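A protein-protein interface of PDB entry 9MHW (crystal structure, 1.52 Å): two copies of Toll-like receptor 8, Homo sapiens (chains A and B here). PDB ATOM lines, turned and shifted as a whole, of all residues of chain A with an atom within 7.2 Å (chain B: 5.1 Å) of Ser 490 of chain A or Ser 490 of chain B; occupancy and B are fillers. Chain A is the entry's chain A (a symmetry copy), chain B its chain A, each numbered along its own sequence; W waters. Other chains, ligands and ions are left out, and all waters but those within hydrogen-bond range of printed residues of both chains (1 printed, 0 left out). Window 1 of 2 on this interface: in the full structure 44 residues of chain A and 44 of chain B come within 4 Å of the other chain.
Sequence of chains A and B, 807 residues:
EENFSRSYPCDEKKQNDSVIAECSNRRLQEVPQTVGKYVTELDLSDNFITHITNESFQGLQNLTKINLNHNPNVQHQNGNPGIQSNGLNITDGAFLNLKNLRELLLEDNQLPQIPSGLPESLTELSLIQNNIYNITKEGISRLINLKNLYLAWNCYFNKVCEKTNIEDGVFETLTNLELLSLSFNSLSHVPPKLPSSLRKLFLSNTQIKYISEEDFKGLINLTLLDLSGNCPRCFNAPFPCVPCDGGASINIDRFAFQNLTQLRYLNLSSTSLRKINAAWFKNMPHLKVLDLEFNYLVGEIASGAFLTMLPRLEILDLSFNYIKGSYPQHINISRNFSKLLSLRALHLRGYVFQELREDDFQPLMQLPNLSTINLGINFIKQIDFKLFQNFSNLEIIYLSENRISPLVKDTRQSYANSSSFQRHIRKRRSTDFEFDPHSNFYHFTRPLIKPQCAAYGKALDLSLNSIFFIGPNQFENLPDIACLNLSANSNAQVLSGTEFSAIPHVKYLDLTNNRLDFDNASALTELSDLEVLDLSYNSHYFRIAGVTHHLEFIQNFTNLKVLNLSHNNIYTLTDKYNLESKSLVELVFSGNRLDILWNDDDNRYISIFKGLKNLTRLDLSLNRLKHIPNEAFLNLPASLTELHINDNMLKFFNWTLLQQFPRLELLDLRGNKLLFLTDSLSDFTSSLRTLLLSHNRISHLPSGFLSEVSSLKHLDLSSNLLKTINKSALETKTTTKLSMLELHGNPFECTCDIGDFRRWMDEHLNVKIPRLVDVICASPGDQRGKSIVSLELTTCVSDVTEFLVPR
NH2 of Arg 515 of chain A is in hydrogen-bond range of O of Asn 465 of chain B, at 2.8 Å.
The guanidinium group of Arg 515 of chain A sits at hydrogen-bond distance from the backbone carbonyl oxygen of Ala 488 of chain B, at 3.2 Å.
The guanidinium group (NH1) of Arg 515 of chain A sits at hydrogen-bond distance from the side-chain hydroxyl (OG) of Ser 490 of chain B, 3.1 Å away.
NH2 of Arg 515 of chain B lies within hydrogen-bond range of O of Asn 465 of chain A, 2.8 Å away.
The guanidinium group (NH2) of Arg 515 of chain B lies within hydrogen-bond range of the backbone carbonyl oxygen (O) of Ala 488 of chain A (3.2 Å).
The guanidinium group (NH1) of Arg 515 of chain B lies within hydrogen-bond range of the side-chain hydroxyl (OG) of Ser 490 of chain A (3.1 Å).
The backbone NH (N) of Asn 465 of chain B lies within hydrogen-bond range of the backbone carbonyl oxygen (O) of Ala 488 of chain B, at 3.4 Å.
The side-chain amide oxygen of Asn 491 of chain B lies close to the backbone carbonyl oxygen of Phe 468 of chain B (3.5 Å).
OD1 of Asn 489 of chain A lies close to O of Asn 465 of chain A, 3.5 Å away.
OD1 of Asn 489 of chain A lies within hydrogen-bond range of N of Ser 466 of chain A (3.3 Å).
The backbone carbonyl oxygen (O) of Asn 513 of chain A sits close to the backbone NH (N) of Ala 488 of chain A, at 3.3 Å.
The backbone NH (N) of Ser 490 of chain A lies within hydrogen-bond range of the side-chain amide oxygen (OD1) of Asn 514 of chain A (3.1 Å).
OG of Ser 466 of chain A touches NH1 of Arg 515 of chain B (3.5 Å).
Phe 468 of chain A touches Phe 468 of chain B (CE2 to CE2, 3.6 Å).
Ser 490 of chain A touches Ser 490 of chain B (OG to CB, 3.5 Å).
Of the printed residues of chain B, Ser 466 of chain A touches Arg 515 (3.5 Å).
Ser 490 of chain A touches just these residues of chain B: Ser 490 and Arg 515.
Of the printed residues of chain B, Arg 515 of chain A touches Asn 465, Ala 488 and Ser 490.
Of the printed residues of chain A, Phe 468 of chain B touches Phe 468 (3.6 Å).
Ser 490 of chain B touches just these residues of chain A: Ser 490 and Arg 515.
The nearest printed residue of chain B that does not touch Ser 490 of chain A is Asn 491 of chain B (6.2 Å).
The nearest printed residue of chain B that does not touch Phe 468 of chain A is Ser 490 of chain B (6.6 Å).
Hydrophobic or aromatic side chains of chain B that line the printed part of chain A: Phe 468.
Of the 18 printed residues of chain A, 6 touch a printed residue of chain B.
Among the printed residues, 9 pairs touch across the chains.
Among the printed residues, no Asp or Glu carboxylate lies within 4 Å of a Lys or Arg side-chain nitrogen of the other chain.
Asn 465 of chain A touches Arg 515 of chain B, and with the chains exchanged Arg 515 of chain A touches Asn 465 of chain B.
Phe 468 of chain A touches its own counterpart, Phe 468 of chain B.
Ser 490 of chain A touches its own counterpart, Ser 490 of chain B.
Ser 490 of chain A touches Arg 515 of chain B, and with the chains exchanged Arg 515 of chain A touches Ser 490 of chain B.
10 positions are printed for both chains.
Water W1 lies within hydrogen-bond range of O of Ser 490 of chain B (2.8 Å), NH1 of Arg 515 of chain B (2.9 Å) and OG of Ser 466 of chain A (3.3 Å).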
ATOM      1  N   ASN A 465     -14.866  -4.707  25.461  1.00  0.00           N
ATOM      2  CA  ASN A 465     -14.528  -3.292  25.459  1.00  0.00           C
ATOM      3  C   ASN A 465     -13.751  -3.041  24.141  1.00  0.00           C
ATOM      4  O   ASN A 465     -13.862  -3.849  23.221  1.00  0.00           O
ATOM      5  CB  ASN A 465     -13.759  -2.960  26.767  1.00  0.00           C
ATOM      6  CG  ASN A 465     -14.690  -2.614  27.895  1.00  0.00           C
ATOM      7  OD1 ASN A 465     -15.338  -1.574  27.841  1.00  0.00           O
ATOM      8  ND2 ASN A 465     -14.831  -3.480  28.900  1.00  0.00           N
ATOM      9  N   SER A 466     -13.034  -1.931  24.008  1.00  0.00           N
ATOM     10  CA  SER A 466     -12.263  -1.604  22.804  1.00  0.00           C
ATOM     11  C   SER A 466     -10.801  -1.273  23.168  1.00  0.00           C
ATOM     12  O   SER A 466     -10.229  -0.334  22.611  1.00  0.00           O
ATOM     13  CB  SER A 466     -12.920  -0.422  22.100  1.00  0.00           C
ATOM     14  OG  SER A 466     -14.239  -0.777  21.726  1.00  0.00           O
ATOM     15  N   ILE A 467     -10.181  -2.049  24.079  1.00  0.00           N
ATOM     16  CA  ILE A 467      -8.771  -1.834  24.448  1.00  0.00           C
ATOM     17  C   ILE A 467      -7.979  -2.592  23.386  1.00  0.00           C
ATOM     18  O   ILE A 467      -7.471  -3.696  23.614  1.00  0.00           O
ATOM     19  CB  ILE A 467      -8.452  -2.282  25.903  1.00  0.00           C
ATOM     20  CG1 ILE A 467      -9.425  -1.599  26.903  1.00  0.00           C
ATOM     21  CG2 ILE A 467      -7.000  -1.936  26.278  1.00  0.00           C
ATOM     22  CD1 ILE A 467      -9.314  -2.160  28.338  1.00  0.00           C
ATOM     23  N   PHE A 468      -7.969  -2.015  22.184  1.00  0.00           N
ATOM     24  CA  PHE A 468      -7.364  -2.638  21.014  1.00  0.00           C
ATOM     25  C   PHE A 468      -5.838  -2.691  21.040  1.00  0.00           C
ATOM     26  O   PHE A 468      -5.242  -3.398  20.217  1.00  0.00           O
ATOM     27  CB  PHE A 468      -7.857  -1.968  19.717  1.00  0.00           C
ATOM     28  CG  PHE A 468      -7.486  -0.512  19.557  1.00  0.00           C
ATOM     29  CD1 PHE A 468      -6.250  -0.147  19.052  1.00  0.00           C
ATOM     30  CD2 PHE A 468      -8.397   0.488  19.855  1.00  0.00           C
ATOM     31  CE1 PHE A 468      -5.913   1.193  18.897  1.00  0.00           C
ATOM     32  CE2 PHE A 468      -8.068   1.828  19.668  1.00  0.00           C
ATOM     33  CZ  PHE A 468      -6.823   2.172  19.207  1.00  0.00           C
ATOM     34  N   PHE A 469      -5.208  -1.917  21.932  1.00  0.00           N
ATOM     35  CA  PHE A 469      -3.761  -1.849  22.057  1.00  0.00           C
ATOM     36  C   PHE A 469      -3.445  -1.517  23.508  1.00  0.00           C
ATOM     37  O   PHE A 469      -4.017  -0.573  24.053  1.00  0.00           O
ATOM     38  CB  PHE A 469      -3.197  -0.746  21.129  1.00  0.00           C
ATOM     39  CG  PHE A 469      -1.707  -0.538  21.273  1.00  0.00           C
ATOM     40  CD1 PHE A 469      -0.809  -1.406  20.675  1.00  0.00           C
ATOM     41  CD2 PHE A 469      -1.204   0.531  21.997  1.00  0.00           C
ATOM     42  CE1 PHE A 469       0.559  -1.229  20.828  1.00  0.00           C
ATOM     43  CE2 PHE A 469       0.168   0.707  22.147  1.00  0.00           C
ATOM     44  CZ  PHE A 469       1.039  -0.174  21.567  1.00  0.00           C
ATOM     45  N   LEU A 486      -9.488  -9.962  29.277  1.00  0.00           N
ATOM     46  CA  LEU A 486      -9.410  -9.010  28.181  1.00  0.00           C
ATOM     47  C   LEU A 486     -10.040  -9.604  26.906  1.00  0.00           C
ATOM     48  O   LEU A 486      -9.738  -9.149  25.809  1.00  0.00           O
ATOM     49  CB  LEU A 486      -7.949  -8.621  27.943  1.00  0.00           C
ATOM     50  CG  LEU A 486      -7.329  -7.669  28.973  1.00  0.00           C
ATOM     51  CD1 LEU A 486      -5.808  -7.667  28.844  1.00  0.00           C
ATOM     52  CD2 LEU A 486      -7.872  -6.234  28.813  1.00  0.00           C
ATOM     53  N   SER A 487     -10.973 -10.550  27.050  1.00  0.00           N
ATOM     54  CA  SER A 487     -11.643 -11.159  25.911  1.00  0.00           C
ATOM     55  C   SER A 487     -12.398 -10.123  25.110  1.00  0.00           C
ATOM     56  O   SER A 487     -12.944  -9.186  25.686  1.00  0.00           O
ATOM     57  CB  SER A 487     -12.649 -12.208  26.376  1.00  0.00           C
ATOM     58  OG  SER A 487     -13.305 -12.827  25.278  1.00  0.00           O
ATOM     59  N   ALA A 488     -12.463 -10.303  23.795  1.00  0.00           N
ATOM     60  CA  ALA A 488     -13.275  -9.448  22.932  1.00  0.00           C
ATOM     61  C   ALA A 488     -13.003  -7.940  23.096  1.00  0.00           C
ATOM     62  O   ALA A 488     -13.911  -7.172  23.394  1.00  0.00           O
ATOM     63  CB  ALA A 488     -14.761  -9.767  23.130  1.00  0.00           C
ATOM     64  N   ASN A 489     -11.750  -7.535  22.885  1.00  0.00           N
ATOM     65  CA  ASN A 489     -11.329  -6.134  22.901  1.00  0.00           C
ATOM     66  C   ASN A 489     -10.773  -5.677  21.539  1.00  0.00           C
ATOM     67  O   ASN A 489     -10.201  -4.590  21.453  1.00  0.00           O
ATOM     68  CB  ASN A 489     -10.291  -5.912  24.021  1.00  0.00           C
ATOM     69  CG  ASN A 489     -10.968  -5.513  25.306  1.00  0.00           C
ATOM     70  OD1 ASN A 489     -11.288  -4.346  25.484  1.00  0.00           O
ATOM     71  ND2 ASN A 489     -11.295  -6.483  26.145  1.00  0.00           N
ATOM     72  N   SER A 490     -10.961  -6.476  20.472  1.00  0.00           N
ATOM     73  CA  SER A 490     -10.443  -6.146  19.136  1.00  0.00           C
ATOM     74  C   SER A 490      -8.930  -5.929  19.157  1.00  0.00           C
ATOM     75  O   SER A 490      -8.413  -5.149  18.357  1.00  0.00           O
ATOM     76  CB  SER A 490     -11.136  -4.897  18.605  1.00  0.00           C
ATOM     77  OG  SER A 490     -12.538  -5.086  18.559  1.00  0.00           O
ATOM     78  N   ASN A 491      -8.215  -6.633  20.055  1.00  0.00           N
ATOM     79  CA  ASN A 491      -6.791  -6.429  20.200  1.00  0.00           C
ATOM     80  C   ASN A 491      -6.031  -7.166  19.122  1.00  0.00           C
ATOM     81  O   ASN A 491      -6.070  -8.380  19.074  1.00  0.00           O
ATOM     82  CB  ASN A 491      -6.319  -6.844  21.592  1.00  0.00           C
ATOM     83  CG  ASN A 491      -4.923  -6.342  21.897  1.00  0.00           C
ATOM     84  OD1 ASN A 491      -4.000  -6.510  21.103  1.00  0.00           O
ATOM     85  ND2 ASN A 491      -4.721  -5.689  23.028  1.00  0.00           N
ATOM     86  N   ALA A 492      -5.317  -6.426  18.282  1.00  0.00           N
ATOM     87  CA  ALA A 492      -4.530  -6.986  17.194  1.00  0.00           C
ATOM     88  C   ALA A 492      -3.028  -6.713  17.372  1.00  0.00           C
ATOM     89  O   ALA A 492      -2.287  -6.761  16.390  1.00  0.00           O
ATOM     90  CB  ALA A 492      -5.011  -6.379  15.887  1.00  0.00           C
ATOM     91  N   GLN A 493      -2.559  -6.479  18.604  1.00  0.00           N
ATOM     92  CA  GLN A 493      -1.165  -6.115  18.817  1.00  0.00           C
ATOM     93  C   GLN A 493      -0.246  -7.334  18.890  1.00  0.00           C
ATOM     94  O   GLN A 493      -0.698  -8.468  19.076  1.00  0.00           O
ATOM     95  CB  GLN A 493      -1.039  -5.222  20.086  1.00  0.00           C
ATOM     96  CG  GLN A 493      -0.757  -5.972  21.394  1.00  0.00           C
ATOM     97  CD  GLN A 493      -0.873  -5.024  22.546  1.00  0.00           C
ATOM     98  OE1 GLN A 493      -1.923  -4.920  23.160  1.00  0.00           O
ATOM     99  NE2 GLN A 493       0.185  -4.269  22.827  1.00  0.00           N
ATOM    100  N   THR A 512      -9.177 -14.373  24.928  1.00  0.00           N
ATOM    101  CA  THR A 512      -9.956 -14.966  23.860  1.00  0.00           C
ATOM    102  C   THR A 512     -10.668 -13.938  23.009  1.00  0.00           C
ATOM    103  O   THR A 512     -10.972 -12.850  23.475  1.00  0.00           O
ATOM    104  CB  THR A 512     -10.995 -15.940  24.423  1.00  0.00           C
ATOM    105  OG1 THR A 512     -11.969 -15.205  25.173  1.00  0.00           O
ATOM    106  CG2 THR A 512     -10.383 -17.031  25.305  1.00  0.00           C
ATOM    107  N   ASN A 513     -10.977 -14.307  21.767  1.00  0.00           N
ATOM    108  CA  ASN A 513     -11.817 -13.495  20.901  1.00  0.00           C
ATOM    109  C   ASN A 513     -11.225 -12.140  20.636  1.00  0.00           C
ATOM    110  O   ASN A 513     -11.906 -11.126  20.699  1.00  0.00           O
ATOM    111  CB  ASN A 513     -13.248 -13.417  21.448  1.00  0.00           C
ATOM    112  CG  ASN A 513     -13.914 -14.769  21.471  1.00  0.00           C
ATOM    113  OD1 ASN A 513     -14.469 -15.223  20.470  1.00  0.00           O
ATOM    114  ND2 ASN A 513     -13.856 -15.462  22.592  1.00  0.00           N
ATOM    115  N   ASN A 514      -9.955 -12.134  20.264  1.00  0.00           N
ATOM    116  CA  ASN A 514      -9.255 -10.922  19.844  1.00  0.00           C
ATOM    117  C   ASN A 514      -8.673 -11.233  18.446  1.00  0.00           C
ATOM    118  O   ASN A 514      -9.092 -12.196  17.802  1.00  0.00           O
ATOM    119  CB  ASN A 514      -8.178 -10.545  20.906  1.00  0.00           C
ATOM    120  CG  ASN A 514      -8.777  -9.809  22.088  1.00  0.00           C
ATOM    121  OD1 ASN A 514      -9.297  -8.692  21.930  1.00  0.00           O
ATOM    122  ND2 ASN A 514      -8.717 -10.394  23.278  1.00  0.00           N
ATOM    123  N   ARG A 515      -7.793 -10.380  17.945  1.00  0.00           N
ATOM    124  CA  ARG A 515      -7.103 -10.570  16.676  1.00  0.00           C
ATOM    125  C   ARG A 515      -5.594 -10.552  16.981  1.00  0.00           C
ATOM    126  O   ARG A 515      -4.820  -9.993  16.189  1.00  0.00           O
ATOM    127  CB  ARG A 515      -7.448  -9.400  15.739  1.00  0.00           C
ATOM    128  CG  ARG A 515      -8.924  -9.165  15.530  1.00  0.00           C
ATOM    129  CD  ARG A 515      -9.175  -7.780  14.977  1.00  0.00           C
ATOM    130  NE  ARG A 515      -9.054  -7.716  13.523  1.00  0.00           N
ATOM    131  CZ  ARG A 515      -9.064  -6.585  12.815  1.00  0.00           C
ATOM    132  NH1 ARG A 515      -9.126  -5.400  13.430  1.00  0.00           N
ATOM    133  NH2 ARG A 515      -8.969  -6.624  11.491  1.00  0.00           N
ATOM    134  N   LEU A 516      -5.156 -11.149  18.128  1.00  0.00           N
ATOM    135  CA  LEU A 516      -3.754 -11.060  18.508  1.00  0.00           C
ATOM    136  C   LEU A 516      -2.801 -11.608  17.459  1.00  0.00           C
ATOM    137  O   LEU A 516      -3.075 -12.615  16.807  1.00  0.00           O
ATOM    138  CB  LEU A 516      -3.488 -11.743  19.834  1.00  0.00           C
ATOM    139  CG  LEU A 516      -4.037 -11.032  21.063  1.00  0.00           C
ATOM    140  CD1 LEU A 516      -4.039 -11.993  22.246  1.00  0.00           C
ATOM    141  CD2 LEU A 516      -3.202  -9.779  21.391  1.00  0.00           C
ATOM    142  N   ASN B 465      -8.935  -4.570   8.391  1.00  0.00           N
ATOM    143  CA  ASN B 465      -8.125  -3.437   8.811  1.00  0.00           C
ATOM    144  C   ASN B 465      -8.621  -3.063  10.232  1.00  0.00           C
ATOM    145  O   ASN B 465      -9.249  -3.897  10.882  1.00  0.00           O
ATOM    146  CB  ASN B 465      -8.240  -2.315   7.742  1.00  0.00           C
ATOM    147  CG  ASN B 465      -7.227  -2.479   6.644  1.00  0.00           C
ATOM    148  OD1 ASN B 465      -6.037  -2.316   6.896  1.00  0.00           O
ATOM    149  ND2 ASN B 465      -7.645  -2.856   5.435  1.00  0.00           N
ATOM    150  N   PHE B 468     -11.981   1.290  13.073  1.00  0.00           N
ATOM    151  CA  PHE B 468     -12.985   1.030  14.098  1.00  0.00           C
ATOM    152  C   PHE B 468     -14.043   2.120  14.243  1.00  0.00           C
ATOM    153  O   PHE B 468     -15.060   1.894  14.913  1.00  0.00           O
ATOM    154  CB  PHE B 468     -12.319   0.742  15.458  1.00  0.00           C
ATOM    155  CG  PHE B 468     -11.521   1.883  16.046  1.00  0.00           C
ATOM    156  CD1 PHE B 468     -12.143   2.881  16.775  1.00  0.00           C
ATOM    157  CD2 PHE B 468     -10.142   1.921  15.918  1.00  0.00           C
ATOM    158  CE1 PHE B 468     -11.407   3.925  17.322  1.00  0.00           C
ATOM    159  CE2 PHE B 468      -9.405   2.951  16.495  1.00  0.00           C
ATOM    160  CZ  PHE B 468     -10.043   3.955  17.178  1.00  0.00           C
ATOM    161  N   ALA B 488     -14.843  -6.762   8.776  1.00  0.00           N
ATOM    162  CA  ALA B 488     -13.777  -7.051   9.732  1.00  0.00           C
ATOM    163  C   ALA B 488     -12.835  -5.863  10.011  1.00  0.00           C
ATOM    164  O   ALA B 488     -11.628  -5.967   9.822  1.00  0.00           O
ATOM    165  CB  ALA B 488     -12.990  -8.286   9.278  1.00  0.00           C
ATOM    166  N   ASN B 489     -13.404  -4.749  10.472  1.00  0.00           N
ATOM    167  CA  ASN B 489     -12.658  -3.559  10.882  1.00  0.00           C
ATOM    168  C   ASN B 489     -12.861  -3.229  12.373  1.00  0.00           C
ATOM    169  O   ASN B 489     -12.459  -2.153  12.815  1.00  0.00           O
ATOM    170  CB  ASN B 489     -13.057  -2.359   9.995  1.00  0.00           C
ATOM    171  CG  ASN B 489     -12.156  -2.262   8.793  1.00  0.00           C
ATOM    172  OD1 ASN B 489     -11.066  -1.718   8.896  1.00  0.00           O
ATOM    173  ND2 ASN B 489     -12.546  -2.885   7.691  1.00  0.00           N
ATOM    174  N   SER B 490     -13.448  -4.154  13.157  1.00  0.00           N
ATOM    175  CA  SER B 490     -13.714  -3.925  14.585  1.00  0.00           C
ATOM    176  C   SER B 490     -14.568  -2.675  14.805  1.00  0.00           C
ATOM    177  O   SER B 490     -14.439  -2.022  15.840  1.00  0.00           O
ATOM    178  CB  SER B 490     -12.400  -3.792  15.343  1.00  0.00           C
ATOM    179  OG  SER B 490     -11.604  -4.949  15.167  1.00  0.00           O
ATOM    180  N   ASN B 491     -15.454  -2.352  13.845  1.00  0.00           N
ATOM    181  CA  ASN B 491     -16.242  -1.144  13.932  1.00  0.00           C
ATOM    182  C   ASN B 491     -17.421  -1.337  14.856  1.00  0.00           C
ATOM    183  O   ASN B 491     -18.289  -2.139  14.573  1.00  0.00           O
ATOM    184  CB  ASN B 491     -16.694  -0.686  12.546  1.00  0.00           C
ATOM    185  CG  ASN B 491     -17.226   0.733  12.557  1.00  0.00           C
ATOM    186  OD1 ASN B 491     -18.064   1.091  13.383  1.00  0.00           O
ATOM    187  ND2 ASN B 491     -16.747   1.593  11.675  1.00  0.00           N
ATOM    188  N   ALA B 492     -17.459  -0.575  15.944  1.00  0.00           N
ATOM    189  CA  ALA B 492     -18.528  -0.641  16.929  1.00  0.00           C
ATOM    190  C   ALA B 492     -19.313   0.678  17.012  1.00  0.00           C
ATOM    191  O   ALA B 492     -19.964   0.927  18.028  1.00  0.00           O
ATOM    192  CB  ALA B 492     -17.918  -0.963  18.282  1.00  0.00           C
ATOM    193  N   ASN B 513     -19.016  -8.724   9.822  1.00  0.00           N
ATOM    194  CA  ASN B 513     -17.962  -9.062  10.766  1.00  0.00           C
ATOM    195  C   ASN B 513     -17.399  -7.850  11.454  1.00  0.00           C
ATOM    196  O   ASN B 513     -16.192  -7.697  11.582  1.00  0.00           O
ATOM    197  CB  ASN B 513     -16.879  -9.914  10.092  1.00  0.00           C
ATOM    198  CG  ASN B 513     -17.420 -11.243   9.627  1.00  0.00           C
ATOM    199  OD1 ASN B 513     -17.501 -12.202  10.397  1.00  0.00           O
ATOM    200  ND2 ASN B 513     -17.832 -11.335   8.378  1.00  0.00           N
ATOM    201  N   ASN B 514     -18.290  -7.016  11.963  1.00  0.00           N
ATOM    202  CA  ASN B 514     -17.923  -5.857  12.773  1.00  0.00           C
ATOM    203  C   ASN B 514     -18.709  -6.000  14.096  1.00  0.00           C
ATOM    204  O   ASN B 514     -19.211  -7.082  14.404  1.00  0.00           O
ATOM    205  CB  ASN B 514     -18.241  -4.549  11.989  1.00  0.00           C
ATOM    206  CG  ASN B 514     -17.158  -4.210  10.983  1.00  0.00           C
ATOM    207  OD1 ASN B 514     -16.010  -3.933  11.371  1.00  0.00           O
ATOM    208  ND2 ASN B 514     -17.483  -4.214   9.696  1.00  0.00           N
ATOM    209  N   ARG B 515     -18.734  -4.955  14.909  1.00  0.00           N
ATOM    210  CA  ARG B 515     -19.489  -4.908  16.155  1.00  0.00           C
ATOM    211  C   ARG B 515     -20.451  -3.710  16.050  1.00  0.00           C
ATOM    212  O   ARG B 515     -20.656  -3.005  17.050  1.00  0.00           O
ATOM    213  CB  ARG B 515     -18.514  -4.679  17.322  1.00  0.00           C
ATOM    214  CG  ARG B 515     -17.378  -5.669  17.408  1.00  0.00           C
ATOM    215  CD  ARG B 515     -16.262  -5.132  18.277  1.00  0.00           C
ATOM    216  NE  ARG B 515     -16.471  -5.392  19.698  1.00  0.00           N
ATOM    217  CZ  ARG B 515     -15.722  -4.880  20.676  1.00  0.00           C
ATOM    218  NH1 ARG B 515     -14.738  -4.020  20.397  1.00  0.00           N
ATOM    219  NH2 ARG B 515     -15.974  -5.189  21.943  1.00  0.00           N
HETATM  220  O   HOH W   1     -14.259  -1.821  18.584  1.00  0.00           O
